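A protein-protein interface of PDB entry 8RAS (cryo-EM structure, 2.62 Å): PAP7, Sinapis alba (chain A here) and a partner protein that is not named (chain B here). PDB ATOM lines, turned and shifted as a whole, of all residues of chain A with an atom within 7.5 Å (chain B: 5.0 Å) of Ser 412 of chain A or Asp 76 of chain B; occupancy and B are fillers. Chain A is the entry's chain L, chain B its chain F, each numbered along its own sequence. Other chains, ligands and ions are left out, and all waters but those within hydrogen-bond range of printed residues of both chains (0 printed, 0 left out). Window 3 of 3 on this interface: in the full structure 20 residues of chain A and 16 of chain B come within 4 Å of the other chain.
Among the printed residues, pairs that only touch across the chains: Pro 409 of chain A with Met 79 of chain B, Ile 410 of chain A with Asp 76 of chain B, Ile 410 of chain A with Met 79 of chain B, Ile 410 of chain A with Glu 80 of chain B, Pro 411 of chain A with Leu 72 of chain B, Pro 411 of chain A with Met 75 of chain B and Pro 411 of chain A with Asp 76 of chain B.
Of the 12 printed residues of chain A, 4 touch a printed residue of chain B. Printed residues of chain A that touch a printed residue of chain B: Pro 409, Ile 410, Pro 411 and Ser 412. Hydrophobic or aromatic side chains of chain A within 4 Å of the printed part of chain B: Ile 410 and Pro 411. Hydrophobic or aromatic side chains of chain B that line the printed part of chain A: Leu 72, Met 75 and Met 79. Along chain B the printed residues that touch a printed residue of chain A span positions 72 to 80. Among the printed residues, 8 pairs touch across the chains. Among the printed residues, no Asp or Glu carboxylate lies within 4 Å of a Lys or Arg side-chain nitrogen of the other chain.
The side-chain carboxylate (OE1) of Glu 414 of chain A sits close to the backbone carbonyl oxygen (O) of Ile 410 of chain A (2.7 Å).
Ser 412 of chain A touches just one residue of chain B: Asp 76. Asp 76 of chain B touches just these residues of chain A: Ile 410 (3.4 Å), Pro 411 (3.6 Å) and Ser 412 (2.2 Å). Of the printed residues of chain B, Pro 411 of chain A touches Leu 72, Met 75 and Asp 76. Of the printed residues of chain B, Ile 410 of chain A touches Asp 76 (3.4 Å), Met 79 (3.7 Å) and Glu 80 (3.8 Å). Of the printed residues of chain A, Leu 72 of chain B touches Pro 411. Printed residues of chain A within 4 Å of Glu 80 of chain B: Ile 410 (3.8 Å). Of the printed residues of chain A, Met 79 of chain B touches Pro 409 (3.8 Å) and Ile 410 (3.7 Å). Phe 74 of chain B touches none of the printed residues of chain A. Leu 78 of chain B touches none of the printed residues of chain A. The nearest printed residue of chain B that does not touch Ser 412 of chain A is Leu 72 of chain B (5.0 Å). The nearest printed residue of chain B that does not touch Ile 410 of chain A is Met 75 of chain B (5.8 Å).
The side-chain hydroxyl of Ser 412 of chain A sits close to the side-chain carboxylate of Asp 76 of chain B, at 2.2 Å.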
ATOM      1  N   PRO A 409     -28.768  26.731   0.576  1.00  0.00           N
ATOM      2  CA  PRO A 409     -29.605  26.076  -0.435  1.00  0.00           C
ATOM      3  C   PRO A 409     -28.916  25.996  -1.787  1.00  0.00           C
ATOM      4  O   PRO A 409     -28.319  26.975  -2.243  1.00  0.00           O
ATOM      5  CB  PRO A 409     -30.841  26.977  -0.485  1.00  0.00           C
ATOM      6  CG  PRO A 409     -30.301  28.346  -0.173  1.00  0.00           C
ATOM      7  CD  PRO A 409     -29.060  28.170   0.683  1.00  0.00           C
ATOM      8  N   ILE A 410     -28.984  24.838  -2.438  1.00  0.00           N
ATOM      9  CA  ILE A 410     -28.471  24.712  -3.800  1.00  0.00           C
ATOM     10  C   ILE A 410     -29.503  25.328  -4.738  1.00  0.00           C
ATOM     11  O   ILE A 410     -30.705  25.064  -4.595  1.00  0.00           O
ATOM     12  CB  ILE A 410     -28.128  23.250  -4.143  1.00  0.00           C
ATOM     13  CG1 ILE A 410     -29.280  22.291  -3.824  1.00  0.00           C
ATOM     14  CG2 ILE A 410     -26.871  22.815  -3.410  1.00  0.00           C
ATOM     15  CD1 ILE A 410     -30.242  22.061  -4.965  1.00  0.00           C
ATOM     16  N   PRO A 411     -29.089  26.183  -5.674  1.00  0.00           N
ATOM     17  CA  PRO A 411     -30.075  26.944  -6.460  1.00  0.00           C
ATOM     18  C   PRO A 411     -31.033  26.088  -7.267  1.00  0.00           C
ATOM     19  O   PRO A 411     -32.185  26.497  -7.462  1.00  0.00           O
ATOM     20  CB  PRO A 411     -29.193  27.810  -7.371  1.00  0.00           C
ATOM     21  CG  PRO A 411     -27.908  27.942  -6.630  1.00  0.00           C
ATOM     22  CD  PRO A 411     -27.711  26.627  -5.936  1.00  0.00           C
ATOM     23  N   SER A 412     -30.608  24.909  -7.731  1.00  0.00           N
ATOM     24  CA  SER A 412     -31.425  24.135  -8.662  1.00  0.00           C
ATOM     25  C   SER A 412     -32.770  23.752  -8.054  1.00  0.00           C
ATOM     26  O   SER A 412     -33.807  23.847  -8.721  1.00  0.00           O
ATOM     27  CB  SER A 412     -30.668  22.887  -9.112  1.00  0.00           C
ATOM     28  OG  SER A 412     -29.447  23.232  -9.740  1.00  0.00           O
ATOM     29  N   ALA A 413     -32.776  23.313  -6.795  1.00  0.00           N
ATOM     30  CA  ALA A 413     -34.043  22.972  -6.155  1.00  0.00           C
ATOM     31  C   ALA A 413     -34.879  24.212  -5.876  1.00  0.00           C
ATOM     32  O   ALA A 413     -36.114  24.140  -5.880  1.00  0.00           O
ATOM     33  CB  ALA A 413     -33.797  22.198  -4.861  1.00  0.00           C
ATOM     34  N   GLU A 414     -34.231  25.354  -5.630  1.00  0.00           N
ATOM     35  CA  GLU A 414     -34.972  26.588  -5.402  1.00  0.00           C
ATOM     36  C   GLU A 414     -35.757  27.009  -6.638  1.00  0.00           C
ATOM     37  O   GLU A 414     -36.909  27.440  -6.525  1.00  0.00           O
ATOM     38  CB  GLU A 414     -34.024  27.701  -4.956  1.00  0.00           C
ATOM     39  CG  GLU A 414     -33.869  27.835  -3.442  1.00  0.00           C
ATOM     40  CD  GLU A 414     -33.766  26.501  -2.727  1.00  0.00           C
ATOM     41  OE1 GLU A 414     -32.854  25.713  -3.050  1.00  0.00           O
ATOM     42  OE2 GLU A 414     -34.601  26.241  -1.835  1.00  0.00           O
ATOM     43  N   ARG A 415     -35.157  26.899  -7.828  1.00  0.00           N
ATOM     44  CA  ARG A 415     -35.878  27.284  -9.039  1.00  0.00           C
ATOM     45  C   ARG A 415     -37.120  26.425  -9.235  1.00  0.00           C
ATOM     46  O   ARG A 415     -38.203  26.943  -9.537  1.00  0.00           O
ATOM     47  CB  ARG A 415     -34.964  27.186 -10.260  1.00  0.00           C
ATOM     48  CG  ARG A 415     -33.518  27.554  -9.999  1.00  0.00           C
ATOM     49  CD  ARG A 415     -33.193  28.938 -10.528  1.00  0.00           C
ATOM     50  NE  ARG A 415     -33.481  29.060 -11.952  1.00  0.00           N
ATOM     51  CZ  ARG A 415     -33.293  30.164 -12.660  1.00  0.00           C
ATOM     52  NH1 ARG A 415     -32.815  31.267 -12.107  1.00  0.00           N
ATOM     53  NH2 ARG A 415     -33.592  30.163 -13.955  1.00  0.00           N
ATOM     54  N   LYS A 416     -36.988  25.111  -9.049  1.00  0.00           N
ATOM     55  CA  LYS A 416     -38.137  24.221  -9.182  1.00  0.00           C
ATOM     56  C   LYS A 416     -39.192  24.518  -8.123  1.00  0.00           C
ATOM     57  O   LYS A 416     -40.397  24.505  -8.412  1.00  0.00           O
ATOM     58  CB  LYS A 416     -37.670  22.767  -9.101  1.00  0.00           C
ATOM     59  CG  LYS A 416     -38.675  21.801  -8.503  1.00  0.00           C
ATOM     60  CD  LYS A 416     -38.232  20.360  -8.705  1.00  0.00           C
ATOM     61  CE  LYS A 416     -36.976  20.049  -7.908  1.00  0.00           C
ATOM     62  NZ  LYS A 416     -37.284  19.698  -6.496  1.00  0.00           N
ATOM     63  N   ALA A 417     -38.759  24.795  -6.890  1.00  0.00           N
ATOM     64  CA  ALA A 417     -39.705  25.087  -5.818  1.00  0.00           C
ATOM     65  C   ALA A 417     -40.494  26.360  -6.108  1.00  0.00           C
ATOM     66  O   ALA A 417     -41.720  26.393  -5.949  1.00  0.00           O
ATOM     67  CB  ALA A 417     -38.966  25.200  -4.486  1.00  0.00           C
ATOM     68  N   VAL A 418     -39.806  27.422  -6.535  1.00  0.00           N
ATOM     69  CA  VAL A 418     -40.516  28.660  -6.839  1.00  0.00           C
ATOM     70  C   VAL A 418     -41.377  28.505  -8.085  1.00  0.00           C
ATOM     71  O   VAL A 418     -42.427  29.142  -8.191  1.00  0.00           O
ATOM     72  CB  VAL A 418     -39.557  29.863  -6.953  1.00  0.00           C
ATOM     73  CG1 VAL A 418     -38.530  29.844  -5.839  1.00  0.00           C
ATOM     74  CG2 VAL A 418     -38.873  29.890  -8.308  1.00  0.00           C
ATOM     75  N   LEU A 481     -30.544  35.013  -6.387  1.00  0.00           N
ATOM     76  CA  LEU A 481     -29.927  33.911  -5.661  1.00  0.00           C
ATOM     77  C   LEU A 481     -28.492  33.646  -6.094  1.00  0.00           C
ATOM     78  O   LEU A 481     -27.798  32.864  -5.435  1.00  0.00           O
ATOM     79  CB  LEU A 481     -30.758  32.637  -5.835  1.00  0.00           C
ATOM     80  CG  LEU A 481     -30.693  31.623  -4.691  1.00  0.00           C
ATOM     81  CD1 LEU A 481     -31.249  32.223  -3.413  1.00  0.00           C
ATOM     82  CD2 LEU A 481     -31.437  30.351  -5.059  1.00  0.00           C
ATOM     83  N   LEU A 482     -28.032  34.275  -7.170  1.00  0.00           N
ATOM     84  CA  LEU A 482     -26.688  34.038  -7.680  1.00  0.00           C
ATOM     85  C   LEU A 482     -25.801  35.262  -7.485  1.00  0.00           C
ATOM     86  O   LEU A 482     -25.772  36.159  -8.327  1.00  0.00           O
ATOM     87  CB  LEU A 482     -26.745  33.654  -9.158  1.00  0.00           C
ATOM     88  CG  LEU A 482     -27.923  32.763  -9.552  1.00  0.00           C
ATOM     89  CD1 LEU A 482     -28.057  32.678 -11.063  1.00  0.00           C
ATOM     90  CD2 LEU A 482     -27.776  31.376  -8.944  1.00  0.00           C
ATOM     91  N   ARG B  71     -23.250  31.274 -14.188  1.00  0.00           N
ATOM     92  CA  ARG B  71     -23.281  31.563 -12.761  1.00  0.00           C
ATOM     93  C   ARG B  71     -24.172  30.578 -12.021  1.00  0.00           C
ATOM     94  O   ARG B  71     -23.853  30.170 -10.902  1.00  0.00           O
ATOM     95  CB  ARG B  71     -23.755  32.997 -12.523  1.00  0.00           C
ATOM     96  CG  ARG B  71     -22.678  34.045 -12.734  1.00  0.00           C
ATOM     97  CD  ARG B  71     -23.147  35.412 -12.269  1.00  0.00           C
ATOM     98  NE  ARG B  71     -22.057  36.378 -12.225  1.00  0.00           N
ATOM     99  CZ  ARG B  71     -21.153  36.446 -11.257  1.00  0.00           C
ATOM    100  NH1 ARG B  71     -21.175  35.611 -10.231  1.00  0.00           N
ATOM    101  NH2 ARG B  71     -20.204  37.376 -11.319  1.00  0.00           N
ATOM    102  N   LEU B  72     -25.291  30.180 -12.628  1.00  0.00           N
ATOM    103  CA  LEU B  72     -26.173  29.205 -11.996  1.00  0.00           C
ATOM    104  C   LEU B  72     -25.465  27.872 -11.805  1.00  0.00           C
ATOM    105  O   LEU B  72     -25.506  27.285 -10.717  1.00  0.00           O
ATOM    106  CB  LEU B  72     -27.437  29.023 -12.833  1.00  0.00           C
ATOM    107  CG  LEU B  72     -28.361  27.884 -12.401  1.00  0.00           C
ATOM    108  CD1 LEU B  72     -29.052  28.220 -11.091  1.00  0.00           C
ATOM    109  CD2 LEU B  72     -29.378  27.576 -13.488  1.00  0.00           C
ATOM    110  N   THR B  73     -24.799  27.383 -12.852  1.00  0.00           N
ATOM    111  CA  THR B  73     -24.094  26.108 -12.747  1.00  0.00           C
ATOM    112  C   THR B  73     -22.984  26.183 -11.707  1.00  0.00           C
ATOM    113  O   THR B  73     -22.836  25.285 -10.863  1.00  0.00           O
ATOM    114  CB  THR B  73     -23.523  25.708 -14.107  1.00  0.00           C
ATOM    115  OG1 THR B  73     -22.801  26.813 -14.665  1.00  0.00           O
ATOM    116  CG2 THR B  73     -24.639  25.311 -15.058  1.00  0.00           C
ATOM    117  N   PHE B  74     -22.200  27.264 -11.742  1.00  0.00           N
ATOM    118  CA  PHE B  74     -21.074  27.384 -10.824  1.00  0.00           C
ATOM    119  C   PHE B  74     -21.553  27.527  -9.385  1.00  0.00           C
ATOM    120  O   PHE B  74     -20.981  26.920  -8.474  1.00  0.00           O
ATOM    121  CB  PHE B  74     -20.202  28.568 -11.231  1.00  0.00           C
ATOM    122  CG  PHE B  74     -19.083  28.198 -12.159  1.00  0.00           C
ATOM    123  CD1 PHE B  74     -17.797  28.643 -11.929  1.00  0.00           C
ATOM    124  CD2 PHE B  74     -19.325  27.415 -13.273  1.00  0.00           C
ATOM    125  CE1 PHE B  74     -16.768  28.308 -12.785  1.00  0.00           C
ATOM    126  CE2 PHE B  74     -18.303  27.078 -14.134  1.00  0.00           C
ATOM    127  CZ  PHE B  74     -17.023  27.524 -13.888  1.00  0.00           C
ATOM    128  N   MET B  75     -22.610  28.315  -9.163  1.00  0.00           N
ATOM    129  CA  MET B  75     -23.170  28.468  -7.828  1.00  0.00           C
ATOM    130  C   MET B  75     -23.742  27.157  -7.317  1.00  0.00           C
ATOM    131  O   MET B  75     -23.587  26.826  -6.139  1.00  0.00           O
ATOM    132  CB  MET B  75     -24.251  29.550  -7.834  1.00  0.00           C
ATOM    133  CG  MET B  75     -24.723  29.967  -6.452  1.00  0.00           C
ATOM    134  SD  MET B  75     -23.452  30.821  -5.505  1.00  0.00           S
ATOM    135  CE  MET B  75     -23.150  32.231  -6.565  1.00  0.00           C
ATOM    136  N   ASP B  76     -24.418  26.401  -8.184  1.00  0.00           N
ATOM    137  CA  ASP B  76     -24.957  25.110  -7.770  1.00  0.00           C
ATOM    138  C   ASP B  76     -23.843  24.168  -7.339  1.00  0.00           C
ATOM    139  O   ASP B  76     -23.923  23.533  -6.280  1.00  0.00           O
ATOM    140  CB  ASP B  76     -25.771  24.492  -8.905  1.00  0.00           C
ATOM    141  CG  ASP B  76     -26.655  23.356  -8.433  1.00  0.00           C
ATOM    142  OD1 ASP B  76     -26.677  23.087  -7.214  1.00  0.00           O
ATOM    143  OD2 ASP B  76     -27.318  22.723  -9.280  1.00  0.00           O
ATOM    144  N   GLU B  77     -22.783  24.078  -8.143  1.00  0.00           N
ATOM    145  CA  GLU B  77     -21.705  23.150  -7.817  1.00  0.00           C
ATOM    146  C   GLU B  77     -20.961  23.607  -6.563  1.00  0.00           C
ATOM    147  O   GLU B  77     -20.577  22.782  -5.723  1.00  0.00           O
ATOM    148  CB  GLU B  77     -20.770  23.012  -9.019  1.00  0.00           C
ATOM    149  CG  GLU B  77     -19.996  21.700  -9.113  1.00  0.00           C
ATOM    150  CD  GLU B  77     -18.872  21.578  -8.120  1.00  0.00           C
ATOM    151  OE1 GLU B  77     -18.004  22.470  -8.092  1.00  0.00           O
ATOM    152  OE2 GLU B  77     -18.840  20.570  -7.387  1.00  0.00           O
ATOM    153  N   LEU B  78     -20.775  24.923  -6.403  1.00  0.00           N
ATOM    154  CA  LEU B  78     -20.127  25.461  -5.209  1.00  0.00           C
ATOM    155  C   LEU B  78     -20.953  25.206  -3.954  1.00  0.00           C
ATOM    156  O   LEU B  78     -20.406  24.825  -2.915  1.00  0.00           O
ATOM    157  CB  LEU B  78     -19.883  26.959  -5.381  1.00  0.00           C
ATOM    158  CG  LEU B  78     -19.141  27.679  -4.255  1.00  0.00           C
ATOM    159  CD1 LEU B  78     -18.130  28.663  -4.820  1.00  0.00           C
ATOM    160  CD2 LEU B  78     -20.112  28.387  -3.324  1.00  0.00           C
ATOM    161  N   MET B  79     -22.266  25.441  -4.020  1.00  0.00           N
ATOM    162  CA  MET B  79     -23.122  25.166  -2.874  1.00  0.00           C
ATOM    163  C   MET B  79     -23.141  23.682  -2.553  1.00  0.00           C
ATOM    164  O   MET B  79     -23.206  23.303  -1.377  1.00  0.00           O
ATOM    165  CB  MET B  79     -24.539  25.674  -3.130  1.00  0.00           C
ATOM    166  CG  MET B  79     -24.663  27.186  -3.148  1.00  0.00           C
ATOM    167  SD  MET B  79     -24.344  27.914  -1.533  1.00  0.00           S
ATOM    168  CE  MET B  79     -23.573  29.456  -2.007  1.00  0.00           C
ATOM    169  N   GLU B  80     -23.078  22.832  -3.579  1.00  0.00           N
ATOM    170  CA  GLU B  80     -22.928  21.405  -3.332  1.00  0.00           C
ATOM    171  C   GLU B  80     -21.660  21.128  -2.535  1.00  0.00           C
ATOM    172  O   GLU B  80     -21.717  20.542  -1.450  1.00  0.00           O
ATOM    173  CB  GLU B  80     -22.915  20.643  -4.656  1.00  0.00           C
ATOM    174  CG  GLU B  80     -23.240  19.166  -4.525  1.00  0.00           C
ATOM    175  CD  GLU B  80     -24.359  18.896  -3.539  1.00  0.00           C
ATOM    176  OE1 GLU B  80     -25.538  18.984  -3.940  1.00  0.00           O
ATOM    177  OE2 GLU B  80     -24.061  18.594  -2.363  1.00  0.00           O
